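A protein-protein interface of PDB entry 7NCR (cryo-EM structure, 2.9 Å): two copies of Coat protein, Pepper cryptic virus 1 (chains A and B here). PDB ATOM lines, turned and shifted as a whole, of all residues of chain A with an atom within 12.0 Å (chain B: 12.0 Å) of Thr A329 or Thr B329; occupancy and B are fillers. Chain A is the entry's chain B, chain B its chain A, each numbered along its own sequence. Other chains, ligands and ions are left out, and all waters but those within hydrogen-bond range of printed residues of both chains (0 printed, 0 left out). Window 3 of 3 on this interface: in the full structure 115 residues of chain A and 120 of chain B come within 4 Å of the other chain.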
ATOM      1  N   ALA A 280     -20.265   0.830  -6.473  1.00  0.00           N
ATOM      2  CA  ALA A 280     -20.249   1.830  -7.537  1.00  0.00           C
ATOM      3  C   ALA A 280     -20.921   1.303  -8.799  1.00  0.00           C
ATOM      4  O   ALA A 280     -21.936   1.843  -9.249  1.00  0.00           O
ATOM      5  CB  ALA A 280     -18.809   2.257  -7.829  1.00  0.00           C
ATOM      6  N   LEU A 317     -27.690   9.529  -2.040  1.00  0.00           N
ATOM      7  CA  LEU A 317     -27.324   9.765  -0.654  1.00  0.00           C
ATOM      8  C   LEU A 317     -28.276  10.774  -0.013  1.00  0.00           C
ATOM      9  O   LEU A 317     -28.781  11.678  -0.684  1.00  0.00           O
ATOM     10  CB  LEU A 317     -25.883  10.253  -0.564  1.00  0.00           C
ATOM     11  CG  LEU A 317     -24.889   9.343  -1.283  1.00  0.00           C
ATOM     12  CD1 LEU A 317     -23.482   9.887  -1.172  1.00  0.00           C
ATOM     13  CD2 LEU A 317     -24.961   7.937  -0.723  1.00  0.00           C
ATOM     14  N   SER A 320     -27.519  14.800   3.038  1.00  0.00           N
ATOM     15  CA  SER A 320     -26.648  15.324   4.082  1.00  0.00           C
ATOM     16  C   SER A 320     -25.186  15.055   3.754  1.00  0.00           C
ATOM     17  O   SER A 320     -24.341  15.950   3.869  1.00  0.00           O
ATOM     18  CB  SER A 320     -27.020  14.718   5.433  1.00  0.00           C
ATOM     19  OG  SER A 320     -26.095  15.104   6.432  1.00  0.00           O
ATOM     20  N   LEU A 321     -24.871  13.827   3.344  1.00  0.00           N
ATOM     21  CA  LEU A 321     -23.526  13.549   2.861  1.00  0.00           C
ATOM     22  C   LEU A 321     -23.233  14.336   1.591  1.00  0.00           C
ATOM     23  O   LEU A 321     -22.077  14.664   1.306  1.00  0.00           O
ATOM     24  CB  LEU A 321     -23.347  12.050   2.627  1.00  0.00           C
ATOM     25  CG  LEU A 321     -23.641  11.161   3.835  1.00  0.00           C
ATOM     26  CD1 LEU A 321     -24.371   9.897   3.415  1.00  0.00           C
ATOM     27  CD2 LEU A 321     -22.357  10.827   4.577  1.00  0.00           C
ATOM     28  N   LEU A 322     -24.274  14.668   0.825  1.00  0.00           N
ATOM     29  CA  LEU A 322     -24.091  15.547  -0.323  1.00  0.00           C
ATOM     30  C   LEU A 322     -23.632  16.929   0.122  1.00  0.00           C
ATOM     31  O   LEU A 322     -22.697  17.499  -0.448  1.00  0.00           O
ATOM     32  CB  LEU A 322     -25.384  15.635  -1.129  1.00  0.00           C
ATOM     33  CG  LEU A 322     -25.840  14.333  -1.784  1.00  0.00           C
ATOM     34  CD1 LEU A 322     -27.010  14.581  -2.716  1.00  0.00           C
ATOM     35  CD2 LEU A 322     -24.692  13.683  -2.531  1.00  0.00           C
ATOM     36  N   ASN A 323     -24.288  17.488   1.141  1.00  0.00           N
ATOM     37  CA  ASN A 323     -23.821  18.736   1.736  1.00  0.00           C
ATOM     38  C   ASN A 323     -22.374  18.605   2.196  1.00  0.00           C
ATOM     39  O   ASN A 323     -21.530  19.468   1.911  1.00  0.00           O
ATOM     40  CB  ASN A 323     -24.719  19.115   2.916  1.00  0.00           C
ATOM     41  CG  ASN A 323     -26.009  19.781   2.488  1.00  0.00           C
ATOM     42  OD1 ASN A 323     -26.390  20.821   3.025  1.00  0.00           O
ATOM     43  ND2 ASN A 323     -26.690  19.188   1.513  1.00  0.00           N
ATOM     44  N   ILE A 324     -22.072  17.512   2.902  1.00  0.00           N
ATOM     45  CA  ILE A 324     -20.754  17.330   3.503  1.00  0.00           C
ATOM     46  C   ILE A 324     -19.672  17.301   2.429  1.00  0.00           C
ATOM     47  O   ILE A 324     -18.599  17.892   2.589  1.00  0.00           O
ATOM     48  CB  ILE A 324     -20.733  16.055   4.365  1.00  0.00           C
ATOM     49  CG1 ILE A 324     -21.552  16.279   5.637  1.00  0.00           C
ATOM     50  CG2 ILE A 324     -19.306  15.635   4.689  1.00  0.00           C
ATOM     51  CD1 ILE A 324     -21.323  15.253   6.710  1.00  0.00           C
ATOM     52  N   ILE A 325     -19.941  16.619   1.315  1.00  0.00           N
ATOM     53  CA  ILE A 325     -18.941  16.553   0.256  1.00  0.00           C
ATOM     54  C   ILE A 325     -18.907  17.852  -0.543  1.00  0.00           C
ATOM     55  O   ILE A 325     -17.861  18.224  -1.087  1.00  0.00           O
ATOM     56  CB  ILE A 325     -19.180  15.324  -0.644  1.00  0.00           C
ATOM     57  CG1 ILE A 325     -20.503  15.433  -1.407  1.00  0.00           C
ATOM     58  CG2 ILE A 325     -19.146  14.045   0.183  1.00  0.00           C
ATOM     59  CD1 ILE A 325     -20.375  15.999  -2.805  1.00  0.00           C
ATOM     60  N   GLU A 326     -20.034  18.564  -0.632  1.00  0.00           N
ATOM     61  CA  GLU A 326     -20.046  19.825  -1.360  1.00  0.00           C
ATOM     62  C   GLU A 326     -19.175  20.863  -0.671  1.00  0.00           C
ATOM     63  O   GLU A 326     -18.375  21.544  -1.323  1.00  0.00           O
ATOM     64  CB  GLU A 326     -21.480  20.329  -1.514  1.00  0.00           C
ATOM     65  CG  GLU A 326     -21.854  20.682  -2.945  1.00  0.00           C
ATOM     66  CD  GLU A 326     -23.350  20.818  -3.142  1.00  0.00           C
ATOM     67  OE1 GLU A 326     -23.994  21.530  -2.343  1.00  0.00           O
ATOM     68  OE2 GLU A 326     -23.879  20.209  -4.096  1.00  0.00           O
ATOM     69  N   ASP A 327     -19.306  21.000   0.652  1.00  0.00           N
ATOM     70  CA  ASP A 327     -18.350  21.849   1.354  1.00  0.00           C
ATOM     71  C   ASP A 327     -17.034  21.127   1.619  1.00  0.00           C
ATOM     72  O   ASP A 327     -16.180  21.663   2.332  1.00  0.00           O
ATOM     73  CB  ASP A 327     -18.943  22.396   2.657  1.00  0.00           C
ATOM     74  CG  ASP A 327     -19.807  21.389   3.381  1.00  0.00           C
ATOM     75  OD1 ASP A 327     -19.273  20.365   3.855  1.00  0.00           O
ATOM     76  OD2 ASP A 327     -21.028  21.633   3.484  1.00  0.00           O
ATOM     77  N   PHE A 328     -16.858  19.924   1.074  1.00  0.00           N
ATOM     78  CA  PHE A 328     -15.569  19.247   1.044  1.00  0.00           C
ATOM     79  C   PHE A 328     -14.850  19.422  -0.287  1.00  0.00           C
ATOM     80  O   PHE A 328     -13.619  19.332  -0.329  1.00  0.00           O
ATOM     81  CB  PHE A 328     -15.750  17.755   1.347  1.00  0.00           C
ATOM     82  CG  PHE A 328     -14.561  16.907   0.996  1.00  0.00           C
ATOM     83  CD1 PHE A 328     -13.450  16.874   1.820  1.00  0.00           C
ATOM     84  CD2 PHE A 328     -14.561  16.130  -0.151  1.00  0.00           C
ATOM     85  CE1 PHE A 328     -12.358  16.089   1.504  1.00  0.00           C
ATOM     86  CE2 PHE A 328     -13.474  15.346  -0.475  1.00  0.00           C
ATOM     87  CZ  PHE A 328     -12.371  15.324   0.354  1.00  0.00           C
ATOM     88  N   THR A 329     -15.582  19.677  -1.368  1.00  0.00           N
ATOM     89  CA  THR A 329     -14.973  19.854  -2.678  1.00  0.00           C
ATOM     90  C   THR A 329     -15.217  21.263  -3.213  1.00  0.00           C
ATOM     91  O   THR A 329     -14.274  22.012  -3.472  1.00  0.00           O
ATOM     92  CB  THR A 329     -15.509  18.830  -3.691  1.00  0.00           C
ATOM     93  OG1 THR A 329     -15.793  17.596  -3.020  1.00  0.00           O
ATOM     94  CG2 THR A 329     -14.486  18.576  -4.780  1.00  0.00           C
ATOM     95  N   LEU B 317     -16.871   7.056   6.926  1.00  0.00           N
ATOM     96  CA  LEU B 317     -17.717   6.508   5.873  1.00  0.00           C
ATOM     97  C   LEU B 317     -17.277   5.072   5.616  1.00  0.00           C
ATOM     98  O   LEU B 317     -16.202   4.671   6.081  1.00  0.00           O
ATOM     99  CB  LEU B 317     -17.633   7.333   4.585  1.00  0.00           C
ATOM    100  CG  LEU B 317     -18.756   8.344   4.321  1.00  0.00           C
ATOM    101  CD1 LEU B 317     -18.872   8.668   2.851  1.00  0.00           C
ATOM    102  CD2 LEU B 317     -20.088   7.869   4.883  1.00  0.00           C
ATOM    103  N   SER B 320     -15.451   1.850   0.726  1.00  0.00           N
ATOM    104  CA  SER B 320     -15.914   1.822  -0.657  1.00  0.00           C
ATOM    105  C   SER B 320     -16.628   3.120  -1.014  1.00  0.00           C
ATOM    106  O   SER B 320     -16.493   3.629  -2.134  1.00  0.00           O
ATOM    107  CB  SER B 320     -16.829   0.621  -0.886  1.00  0.00           C
ATOM    108  OG  SER B 320     -18.189   1.011  -0.862  1.00  0.00           O
ATOM    109  N   LEU B 321     -17.379   3.686  -0.069  1.00  0.00           N
ATOM    110  CA  LEU B 321     -18.006   4.977  -0.319  1.00  0.00           C
ATOM    111  C   LEU B 321     -16.959   6.078  -0.455  1.00  0.00           C
ATOM    112  O   LEU B 321     -17.117   6.994  -1.271  1.00  0.00           O
ATOM    113  CB  LEU B 321     -19.000   5.304   0.797  1.00  0.00           C
ATOM    114  CG  LEU B 321     -20.249   6.079   0.379  1.00  0.00           C
ATOM    115  CD1 LEU B 321     -20.913   5.404  -0.803  1.00  0.00           C
ATOM    116  CD2 LEU B 321     -21.218   6.183   1.538  1.00  0.00           C
ATOM    117  N   LEU B 322     -15.879   6.003   0.329  1.00  0.00           N
ATOM    118  CA  LEU B 322     -14.779   6.948   0.155  1.00  0.00           C
ATOM    119  C   LEU B 322     -14.146   6.798  -1.220  1.00  0.00           C
ATOM    120  O   LEU B 322     -13.818   7.795  -1.876  1.00  0.00           O
ATOM    121  CB  LEU B 322     -13.729   6.745   1.243  1.00  0.00           C
ATOM    122  CG  LEU B 322     -14.119   7.106   2.673  1.00  0.00           C
ATOM    123  CD1 LEU B 322     -12.924   6.948   3.586  1.00  0.00           C
ATOM    124  CD2 LEU B 322     -14.675   8.516   2.747  1.00  0.00           C
ATOM    125  N   ASN B 323     -13.952   5.555  -1.664  1.00  0.00           N
ATOM    126  CA  ASN B 323     -13.467   5.315  -3.018  1.00  0.00           C
ATOM    127  C   ASN B 323     -14.394   5.941  -4.051  1.00  0.00           C
ATOM    128  O   ASN B 323     -13.936   6.481  -5.061  1.00  0.00           O
ATOM    129  CB  ASN B 323     -13.327   3.813  -3.262  1.00  0.00           C
ATOM    130  CG  ASN B 323     -11.908   3.324  -3.077  1.00  0.00           C
ATOM    131  OD1 ASN B 323     -11.621   2.533  -2.179  1.00  0.00           O
ATOM    132  ND2 ASN B 323     -11.005   3.790  -3.933  1.00  0.00           N
ATOM    133  N   ILE B 324     -15.704   5.887  -3.804  1.00  0.00           N
ATOM    134  CA  ILE B 324     -16.660   6.474  -4.741  1.00  0.00           C
ATOM    135  C   ILE B 324     -16.534   7.993  -4.760  1.00  0.00           C
ATOM    136  O   ILE B 324     -16.586   8.620  -5.825  1.00  0.00           O
ATOM    137  CB  ILE B 324     -18.090   6.020  -4.396  1.00  0.00           C
ATOM    138  CG1 ILE B 324     -18.303   4.567  -4.830  1.00  0.00           C
ATOM    139  CG2 ILE B 324     -19.114   6.936  -5.041  1.00  0.00           C
ATOM    140  CD1 ILE B 324     -19.740   4.109  -4.768  1.00  0.00           C
ATOM    141  N   ILE B 325     -16.364   8.612  -3.588  1.00  0.00           N
ATOM    142  CA  ILE B 325     -16.165  10.062  -3.549  1.00  0.00           C
ATOM    143  C   ILE B 325     -14.903  10.452  -4.307  1.00  0.00           C
ATOM    144  O   ILE B 325     -14.892  11.433  -5.062  1.00  0.00           O
ATOM    145  CB  ILE B 325     -16.118  10.586  -2.101  1.00  0.00           C
ATOM    146  CG1 ILE B 325     -17.258  10.022  -1.262  1.00  0.00           C
ATOM    147  CG2 ILE B 325     -16.168  12.103  -2.090  1.00  0.00           C
ATOM    148  CD1 ILE B 325     -16.945  10.008   0.214  1.00  0.00           C
ATOM    149  N   GLU B 326     -13.812   9.709  -4.100  1.00  0.00           N
ATOM    150  CA  GLU B 326     -12.585   9.988  -4.842  1.00  0.00           C
ATOM    151  C   GLU B 326     -12.789   9.820  -6.345  1.00  0.00           C
ATOM    152  O   GLU B 326     -12.324  10.649  -7.135  1.00  0.00           O
ATOM    153  CB  GLU B 326     -11.445   9.101  -4.338  1.00  0.00           C
ATOM    154  CG  GLU B 326     -10.438   9.816  -3.431  1.00  0.00           C
ATOM    155  CD  GLU B 326     -10.753   9.697  -1.951  1.00  0.00           C
ATOM    156  OE1 GLU B 326     -11.945   9.676  -1.590  1.00  0.00           O
ATOM    157  OE2 GLU B 326      -9.804   9.623  -1.143  1.00  0.00           O
ATOM    158  N   ASP B 327     -13.498   8.766  -6.761  1.00  0.00           N
ATOM    159  CA  ASP B 327     -13.780   8.581  -8.181  1.00  0.00           C
ATOM    160  C   ASP B 327     -14.730   9.655  -8.702  1.00  0.00           C
ATOM    161  O   ASP B 327     -14.841   9.853  -9.917  1.00  0.00           O
ATOM    162  CB  ASP B 327     -14.350   7.176  -8.409  1.00  0.00           C
ATOM    163  CG  ASP B 327     -14.675   6.894  -9.869  1.00  0.00           C
ATOM    164  OD1 ASP B 327     -15.622   6.121 -10.127  1.00  0.00           O
ATOM    165  OD2 ASP B 327     -13.975   7.417 -10.758  1.00  0.00           O
ATOM    166  N   PHE B 328     -15.411  10.365  -7.803  1.00  0.00           N
ATOM    167  CA  PHE B 328     -16.282  11.477  -8.161  1.00  0.00           C
ATOM    168  C   PHE B 328     -15.518  12.780  -8.366  1.00  0.00           C
ATOM    169  O   PHE B 328     -16.091  13.741  -8.894  1.00  0.00           O
ATOM    170  CB  PHE B 328     -17.360  11.647  -7.074  1.00  0.00           C
ATOM    171  CG  PHE B 328     -18.157  12.919  -7.175  1.00  0.00           C
ATOM    172  CD1 PHE B 328     -19.181  13.040  -8.096  1.00  0.00           C
ATOM    173  CD2 PHE B 328     -17.889  13.988  -6.336  1.00  0.00           C
ATOM    174  CE1 PHE B 328     -19.917  14.207  -8.185  1.00  0.00           C
ATOM    175  CE2 PHE B 328     -18.622  15.157  -6.422  1.00  0.00           C
ATOM    176  CZ  PHE B 328     -19.638  15.266  -7.345  1.00  0.00           C
ATOM    177  N   THR B 329     -14.240  12.823  -7.991  1.00  0.00           N
ATOM    178  CA  THR B 329     -13.401  14.016  -8.132  1.00  0.00           C
ATOM    179  C   THR B 329     -13.970  15.188  -7.339  1.00  0.00           C
ATOM    180  O   THR B 329     -13.648  15.368  -6.164  1.00  0.00           O
ATOM    181  CB  THR B 329     -13.232  14.436  -9.615  1.00  0.00           C
ATOM    182  OG1 THR B 329     -12.419  13.478 -10.302  1.00  0.00           O
ATOM    183  CG2 THR B 329     -12.589  15.806  -9.715  1.00  0.00           C
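O of Ile A325 lies within hydrogen-bond range of OG1 of Thr A329, 2.9 Å away.
Among the printed residues, pairs that only touch across the chains: Thr A329 with Thr B329 (3.6 Å), Ala A280 with Ile B324 (3.6 Å) and Leu A321 with Leu B317 (3.7 Å).
Among the printed residues, 3 pairs touch across the chains. Among the printed residues, no Asp or Glu carboxylate lies within 4 Å of a Lys or Arg side-chain nitrogen of the other chain.
Leu A321 touches Leu B317, but with the chains exchanged Leu A317 does not touch Leu B321 (4.7 Å). Thr A329 touches its own counterpart, Thr B329. Positions printed for both chains: 317, 320, 321, 322, 323, 324, 325, 326, 327, 328 and 329.
Of the printed residues of chain B, Ala A280 touches Ile B324. Ser A320 touches none of the printed residues of chain B. Printed residues of chain B within 4 Å of Leu A321: Leu B317. No residue of chain B comes within 4 Å of Ile A325. Asp A327 touches none of the printed residues of chain B. No residue of chain B comes within 4 Å of Phe A328. Thr A329 touches just one residue of chain B: Thr B329 (3.6 Å). Of the printed residues of chain A, Leu B317 touches Leu A321 (3.7 Å). Printed residues of chain A within 4 Å of Ile B324: Ala A280 (3.6 Å). Glu B326 touches none of the printed residues of chain A. No residue of chain A comes within 4 Å of Asp B327. No residue of chain A comes within 4 Å of Phe B328. Of the printed residues of chain A, Thr B329 touches Thr A329 (3.6 Å).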
